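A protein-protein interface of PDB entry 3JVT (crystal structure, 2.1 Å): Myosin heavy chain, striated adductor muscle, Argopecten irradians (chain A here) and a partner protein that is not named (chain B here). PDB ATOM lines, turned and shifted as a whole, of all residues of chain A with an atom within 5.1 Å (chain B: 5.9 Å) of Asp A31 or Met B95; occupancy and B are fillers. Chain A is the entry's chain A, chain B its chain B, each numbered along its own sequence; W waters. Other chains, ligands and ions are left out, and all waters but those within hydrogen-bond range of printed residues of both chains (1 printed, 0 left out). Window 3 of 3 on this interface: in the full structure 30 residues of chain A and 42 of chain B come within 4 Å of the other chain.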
ATOM      1  N   TYR A  26     -17.549  -5.548  10.837  1.00  0.00           N
ATOM      2  CA  TYR A  26     -18.734  -6.281  10.384  1.00  0.00           C
ATOM      3  C   TYR A  26     -19.518  -7.068  11.435  1.00  0.00           C
ATOM      4  O   TYR A  26     -20.740  -6.933  11.540  1.00  0.00           O
ATOM      5  CB  TYR A  26     -18.327  -7.223   9.247  1.00  0.00           C
ATOM      6  CG  TYR A  26     -19.502  -7.777   8.475  1.00  0.00           C
ATOM      7  CD1 TYR A  26     -20.348  -6.937   7.772  1.00  0.00           C
ATOM      8  CD2 TYR A  26     -19.773  -9.136   8.469  1.00  0.00           C
ATOM      9  CE1 TYR A  26     -21.441  -7.433   7.082  1.00  0.00           C
ATOM     10  CE2 TYR A  26     -20.863  -9.644   7.786  1.00  0.00           C
ATOM     11  CZ  TYR A  26     -21.694  -8.787   7.097  1.00  0.00           C
ATOM     12  OH  TYR A  26     -22.810  -9.285   6.461  1.00  0.00           O
ATOM     13  N   LYS A  27     -18.815  -7.890  12.201  1.00  0.00           N
ATOM     14  CA  LYS A  27     -19.454  -8.714  13.233  1.00  0.00           C
ATOM     15  C   LYS A  27     -20.203  -7.853  14.257  1.00  0.00           C
ATOM     16  O   LYS A  27     -21.311  -8.201  14.682  1.00  0.00           O
ATOM     17  CB  LYS A  27     -18.386  -9.579  13.921  1.00  0.00           C
ATOM     18  CG  LYS A  27     -18.871 -10.430  15.104  1.00  0.00           C
ATOM     19  CD  LYS A  27     -19.996 -11.379  14.719  1.00  0.00           C
ATOM     20  CE  LYS A  27     -20.384 -12.253  15.910  1.00  0.00           C
ATOM     21  NZ  LYS A  27     -21.802 -12.703  15.849  1.00  0.00           N
ATOM     22  N   LYS A  28     -19.595  -6.733  14.645  1.00  0.00           N
ATOM     23  CA  LYS A  28     -20.227  -5.842  15.609  1.00  0.00           C
ATOM     24  C   LYS A  28     -21.494  -5.243  14.973  1.00  0.00           C
ATOM     25  O   LYS A  28     -22.524  -5.131  15.644  1.00  0.00           O
ATOM     26  CB  LYS A  28     -19.260  -4.731  16.035  1.00  0.00           C
ATOM     27  CG  LYS A  28     -19.812  -3.789  17.123  1.00  0.00           C
ATOM     28  CD  LYS A  28     -18.939  -2.532  17.265  1.00  0.00           C
ATOM     29  CE  LYS A  28     -19.252  -1.717  18.517  1.00  0.00           C
ATOM     30  NZ  LYS A  28     -18.911  -2.449  19.773  1.00  0.00           N
ATOM     31  N   LEU A  29     -21.428  -4.858  13.699  1.00  0.00           N
ATOM     32  CA  LEU A  29     -22.631  -4.313  13.066  1.00  0.00           C
ATOM     33  C   LEU A  29     -23.739  -5.364  13.014  1.00  0.00           C
ATOM     34  O   LEU A  29     -24.916  -5.035  13.196  1.00  0.00           O
ATOM     35  CB  LEU A  29     -22.368  -3.838  11.638  1.00  0.00           C
ATOM     36  CG  LEU A  29     -21.860  -2.436  11.342  1.00  0.00           C
ATOM     37  CD1 LEU A  29     -21.995  -2.245   9.827  1.00  0.00           C
ATOM     38  CD2 LEU A  29     -22.670  -1.369  12.088  1.00  0.00           C
ATOM     39  N   GLN A  30     -23.382  -6.617  12.729  1.00  0.00           N
ATOM     40  CA  GLN A  30     -24.398  -7.690  12.689  1.00  0.00           C
ATOM     41  C   GLN A  30     -25.013  -7.887  14.078  1.00  0.00           C
ATOM     42  O   GLN A  30     -26.232  -7.996  14.217  1.00  0.00           O
ATOM     43  CB  GLN A  30     -23.786  -9.029  12.241  1.00  0.00           C
ATOM     44  CG  GLN A  30     -23.228  -9.041  10.840  1.00  0.00           C
ATOM     45  CD  GLN A  30     -22.761 -10.428  10.420  1.00  0.00           C
ATOM     46  OE1 GLN A  30     -21.975 -11.065  11.122  1.00  0.00           O
ATOM     47  NE2 GLN A  30     -23.238 -10.899   9.262  1.00  0.00           N
ATOM     48  N   ASP A  31     -24.164  -7.936  15.099  1.00  0.00           N
ATOM     49  CA  ASP A  31     -24.654  -8.123  16.472  1.00  0.00           C
ATOM     50  C   ASP A  31     -25.545  -6.958  16.869  1.00  0.00           C
ATOM     51  O   ASP A  31     -26.596  -7.150  17.495  1.00  0.00           O
ATOM     52  CB  ASP A  31     -23.487  -8.203  17.482  1.00  0.00           C
ATOM     53  CG  ASP A  31     -22.682  -9.495  17.352  1.00  0.00           C
ATOM     54  OD1 ASP A  31     -23.265 -10.505  16.927  1.00  0.00           O
ATOM     55  OD2 ASP A  31     -21.484  -9.505  17.694  1.00  0.00           O
ATOM     56  N   GLN A  32     -25.123  -5.743  16.515  1.00  0.00           N
ATOM     57  CA  GLN A  32     -25.918  -4.575  16.878  1.00  0.00           C
ATOM     58  C   GLN A  32     -27.271  -4.515  16.173  1.00  0.00           C
ATOM     59  O   GLN A  32     -28.229  -3.992  16.726  1.00  0.00           O
ATOM     60  CB  GLN A  32     -25.113  -3.282  16.649  1.00  0.00           C
ATOM     61  CG  GLN A  32     -23.984  -3.142  17.671  1.00  0.00           C
ATOM     62  CD  GLN A  32     -23.197  -1.847  17.547  1.00  0.00           C
ATOM     63  OE1 GLN A  32     -22.994  -1.346  16.450  1.00  0.00           O
ATOM     64  NE2 GLN A  32     -22.719  -1.320  18.685  1.00  0.00           N
ATOM     65  N   ARG A  33     -27.348  -5.015  14.940  1.00  0.00           N
ATOM     66  CA  ARG A  33     -28.635  -4.990  14.237  1.00  0.00           C
ATOM     67  C   ARG A  33     -29.576  -5.859  15.021  1.00  0.00           C
ATOM     68  O   ARG A  33     -30.757  -5.541  15.158  1.00  0.00           O
ATOM     69  CB  ARG A  33     -28.477  -5.524  12.818  1.00  0.00           C
ATOM     70  CG  ARG A  33     -29.764  -6.058  12.226  1.00  0.00           C
ATOM     71  CD  ARG A  33     -29.452  -7.342  11.488  1.00  0.00           C
ATOM     72  NE  ARG A  33     -29.476  -7.159  10.054  1.00  0.00           N
ATOM     73  CZ  ARG A  33     -28.820  -7.921   9.187  1.00  0.00           C
ATOM     74  NH1 ARG A  33     -28.925  -7.665   7.896  1.00  0.00           N
ATOM     75  NH2 ARG A  33     -28.041  -8.910   9.603  1.00  0.00           N
ATOM     76  N   ILE A  34     -29.048  -6.960  15.541  1.00  0.00           N
ATOM     77  CA  ILE A  34     -29.870  -7.851  16.338  1.00  0.00           C
ATOM     78  C   ILE A  34     -30.316  -7.108  17.586  1.00  0.00           C
ATOM     79  O   ILE A  34     -31.492  -7.139  17.981  1.00  0.00           O
ATOM     80  CB  ILE A  34     -29.070  -9.092  16.774  1.00  0.00           C
ATOM     81  CG1 ILE A  34     -28.899 -10.041  15.593  1.00  0.00           C
ATOM     82  CG2 ILE A  34     -29.781  -9.798  17.937  1.00  0.00           C
ATOM     83  CD1 ILE A  34     -27.900 -11.155  15.889  1.00  0.00           C
ATOM     84  N   GLY A  35     -29.354  -6.456  18.219  1.00  0.00           N
ATOM     85  CA  GLY A  35     -29.659  -5.695  19.421  1.00  0.00           C
ATOM     86  C   GLY A  35     -30.668  -4.582  19.174  1.00  0.00           C
ATOM     87  O   GLY A  35     -31.634  -4.476  19.917  1.00  0.00           O
ATOM     88  N   ARG B  90     -31.937  -5.984  27.999  1.00  0.00           N
ATOM     89  CA  ARG B  90     -30.834  -5.281  28.632  1.00  0.00           C
ATOM     90  C   ARG B  90     -29.523  -5.481  27.871  1.00  0.00           C
ATOM     91  O   ARG B  90     -28.805  -4.507  27.618  1.00  0.00           O
ATOM     92  CB  ARG B  90     -30.642  -5.727  30.089  1.00  0.00           C
ATOM     93  CG  ARG B  90     -29.677  -4.803  30.823  1.00  0.00           C
ATOM     94  CD  ARG B  90     -29.311  -5.279  32.213  1.00  0.00           C
ATOM     95  NE  ARG B  90     -30.458  -5.334  33.115  1.00  0.00           N
ATOM     96  CZ  ARG B  90     -30.970  -6.461  33.598  1.00  0.00           C
ATOM     97  NH1 ARG B  90     -32.006  -6.421  34.419  1.00  0.00           N
ATOM     98  NH2 ARG B  90     -30.443  -7.632  33.262  1.00  0.00           N
ATOM     99  N   ASN B  91     -29.219  -6.717  27.487  1.00  0.00           N
ATOM    100  CA  ASN B  91     -27.980  -6.977  26.756  1.00  0.00           C
ATOM    101  C   ASN B  91     -28.014  -6.281  25.393  1.00  0.00           C
ATOM    102  O   ASN B  91     -26.977  -5.864  24.875  1.00  0.00           O
ATOM    103  CB  ASN B  91     -27.740  -8.498  26.531  1.00  0.00           C
ATOM    104  CG  ASN B  91     -27.460  -9.273  27.839  1.00  0.00           C
ATOM    105  OD1 ASN B  91     -26.997  -8.703  28.829  1.00  0.00           O
ATOM    106  ND2 ASN B  91     -27.727 -10.587  27.824  1.00  0.00           N
ATOM    107  N   ALA B  92     -29.206  -6.172  24.812  1.00  0.00           N
ATOM    108  CA  ALA B  92     -29.359  -5.535  23.509  1.00  0.00           C
ATOM    109  C   ALA B  92     -28.860  -4.096  23.670  1.00  0.00           C
ATOM    110  O   ALA B  92     -28.045  -3.606  22.875  1.00  0.00           O
ATOM    111  CB  ALA B  92     -30.835  -5.562  23.092  1.00  0.00           C
ATOM    112  N   PHE B  93     -29.371  -3.422  24.686  1.00  0.00           N
ATOM    113  CA  PHE B  93     -28.965  -2.045  24.975  1.00  0.00           C
ATOM    114  C   PHE B  93     -27.450  -1.968  25.273  1.00  0.00           C
ATOM    115  O   PHE B  93     -26.751  -1.081  24.794  1.00  0.00           O
ATOM    116  CB  PHE B  93     -29.727  -1.534  26.194  1.00  0.00           C
ATOM    117  CG  PHE B  93     -31.078  -0.955  25.888  1.00  0.00           C
ATOM    118  CD1 PHE B  93     -32.219  -1.480  26.468  1.00  0.00           C
ATOM    119  CD2 PHE B  93     -31.189   0.194  25.097  1.00  0.00           C
ATOM    120  CE1 PHE B  93     -33.469  -0.865  26.285  1.00  0.00           C
ATOM    121  CE2 PHE B  93     -32.419   0.815  24.905  1.00  0.00           C
ATOM    122  CZ  PHE B  93     -33.558   0.291  25.502  1.00  0.00           C
ATOM    123  N   ALA B  94     -26.956  -2.907  26.067  1.00  0.00           N
ATOM    124  CA  ALA B  94     -25.552  -2.894  26.427  1.00  0.00           C
ATOM    125  C   ALA B  94     -24.642  -3.007  25.208  1.00  0.00           C
ATOM    126  O   ALA B  94     -23.473  -2.634  25.283  1.00  0.00           O
ATOM    127  CB  ALA B  94     -25.262  -4.036  27.451  1.00  0.00           C
ATOM    128  N   MET B  95     -25.165  -3.509  24.091  1.00  0.00           N
ATOM    129  CA  MET B  95     -24.334  -3.630  22.889  1.00  0.00           C
ATOM    130  C   MET B  95     -23.891  -2.284  22.336  1.00  0.00           C
ATOM    131  O   MET B  95     -23.008  -2.214  21.471  1.00  0.00           O
ATOM    132  CB  MET B  95     -25.080  -4.384  21.792  1.00  0.00           C
ATOM    133  CG  MET B  95     -25.243  -5.862  22.034  1.00  0.00           C
ATOM    134  SD  MET B  95     -25.857  -6.561  20.503  1.00  0.00           S
ATOM    135  CE  MET B  95     -27.151  -7.675  21.089  1.00  0.00           C
ATOM    136  N   PHE B  96     -24.533  -1.222  22.801  1.00  0.00           N
ATOM    137  CA  PHE B  96     -24.213   0.127  22.338  1.00  0.00           C
ATOM    138  C   PHE B  96     -23.551   0.913  23.488  1.00  0.00           C
ATOM    139  O   PHE B  96     -23.325   2.117  23.385  1.00  0.00           O
ATOM    140  CB  PHE B  96     -25.510   0.811  21.866  1.00  0.00           C
ATOM    141  CG  PHE B  96     -26.224   0.062  20.746  1.00  0.00           C
ATOM    142  CD1 PHE B  96     -25.834   0.223  19.413  1.00  0.00           C
ATOM    143  CD2 PHE B  96     -27.250  -0.841  21.036  1.00  0.00           C
ATOM    144  CE1 PHE B  96     -26.456  -0.504  18.387  1.00  0.00           C
ATOM    145  CE2 PHE B  96     -27.879  -1.577  20.020  1.00  0.00           C
ATOM    146  CZ  PHE B  96     -27.478  -1.405  18.691  1.00  0.00           C
ATOM    147  N   ASP B  97     -23.220   0.195  24.562  1.00  0.00           N
ATOM    148  CA  ASP B  97     -22.592   0.748  25.765  1.00  0.00           C
ATOM    149  C   ASP B  97     -21.363  -0.120  26.073  1.00  0.00           C
ATOM    150  O   ASP B  97     -21.316  -0.853  27.060  1.00  0.00           O
ATOM    151  CB  ASP B  97     -23.618   0.707  26.913  1.00  0.00           C
ATOM    152  CG  ASP B  97     -23.021   1.077  28.287  1.00  0.00           C
ATOM    153  OD1 ASP B  97     -22.052   1.859  28.363  1.00  0.00           O
ATOM    154  OD2 ASP B  97     -23.565   0.587  29.301  1.00  0.00           O
ATOM    155  N   GLU B  98     -20.358   0.003  25.215  1.00  0.00           N
ATOM    156  CA  GLU B  98     -19.123  -0.750  25.326  1.00  0.00           C
ATOM    157  C   GLU B  98     -18.426  -0.589  26.669  1.00  0.00           C
ATOM    158  O   GLU B  98     -17.943  -1.565  27.243  1.00  0.00           O
ATOM    159  CB  GLU B  98     -18.164  -0.344  24.208  1.00  0.00           C
ATOM    160  CG  GLU B  98     -18.526  -0.891  22.828  1.00  0.00           C
ATOM    161  CD  GLU B  98     -19.892  -0.439  22.336  1.00  0.00           C
ATOM    162  OE1 GLU B  98     -20.891  -1.131  22.633  1.00  0.00           O
ATOM    163  OE2 GLU B  98     -19.968   0.613  21.658  1.00  0.00           O
HETATM  164  O   HOH W   1     -20.771   1.297  18.996  1.00  0.00           O
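Among the printed residues, merely in contact across the chains: Gln A32 with Phe B96, Gly A35 with Ala B92 and Gly A35 with Met B95.
Water W1 lies within hydrogen-bond range of OE2 of Glu B98 (2.9 Å) and NE2 of Gln A32 (3.3 Å).
The side-chain amino group (NZ) of Lys A28 is in salt-bridge range of the side-chain carboxylate (OE1) of Glu B98, 3.7 Å away.
O of Met B95 is in hydrogen-bond range of NE2 of Gln A32, at 2.9 Å.
The backbone carbonyl oxygen of Asp A31 lies close to the side-chain sulfur of Met B95, 3.2 Å away.
Of the printed residues of chain B, Asp A31 touches Met B95.
Met B95 touches three residues of chain A.
Of the printed residues of chain A, Phe B96 touches Gln A32.
Printed residues of chain A within 4 Å of Ala B92: Gly A35 (3.4 Å).
Of the printed residues of chain B, Lys A28 touches Glu B98 (3.4 Å).
Of the printed residues of chain B, Gly A35 touches Ala B92 and Met B95.
Of the printed residues of chain B, Gln A32 touches Met B95 and Phe B96.
The nearest printed residue of chain B that does not touch Asp A31 is Phe B96 (5.9 Å).
The nearest residue of chain A that does not touch Met B95 is Lys A28 (4.4 Å).
The nearest printed residue of chain A that does not touch Glu B98 is Gln A32 (4.4 Å).
Printed residues of chain B that touch a printed residue of chain A: Ala B92, Met B95, Phe B96 and Glu B98.
Hydrophobic or aromatic side chains of chain B that line the printed part of chain A: Ala B92, Met B95 and Phe B96.
O of Met B95 sits close to OE1 of Glu B98, at 2.6 Å.
The side-chain amino group (NZ) of Lys A27 lies within salt-bridge range of the side-chain carboxylate (OD1) of Asp A31, 2.9 Å away.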
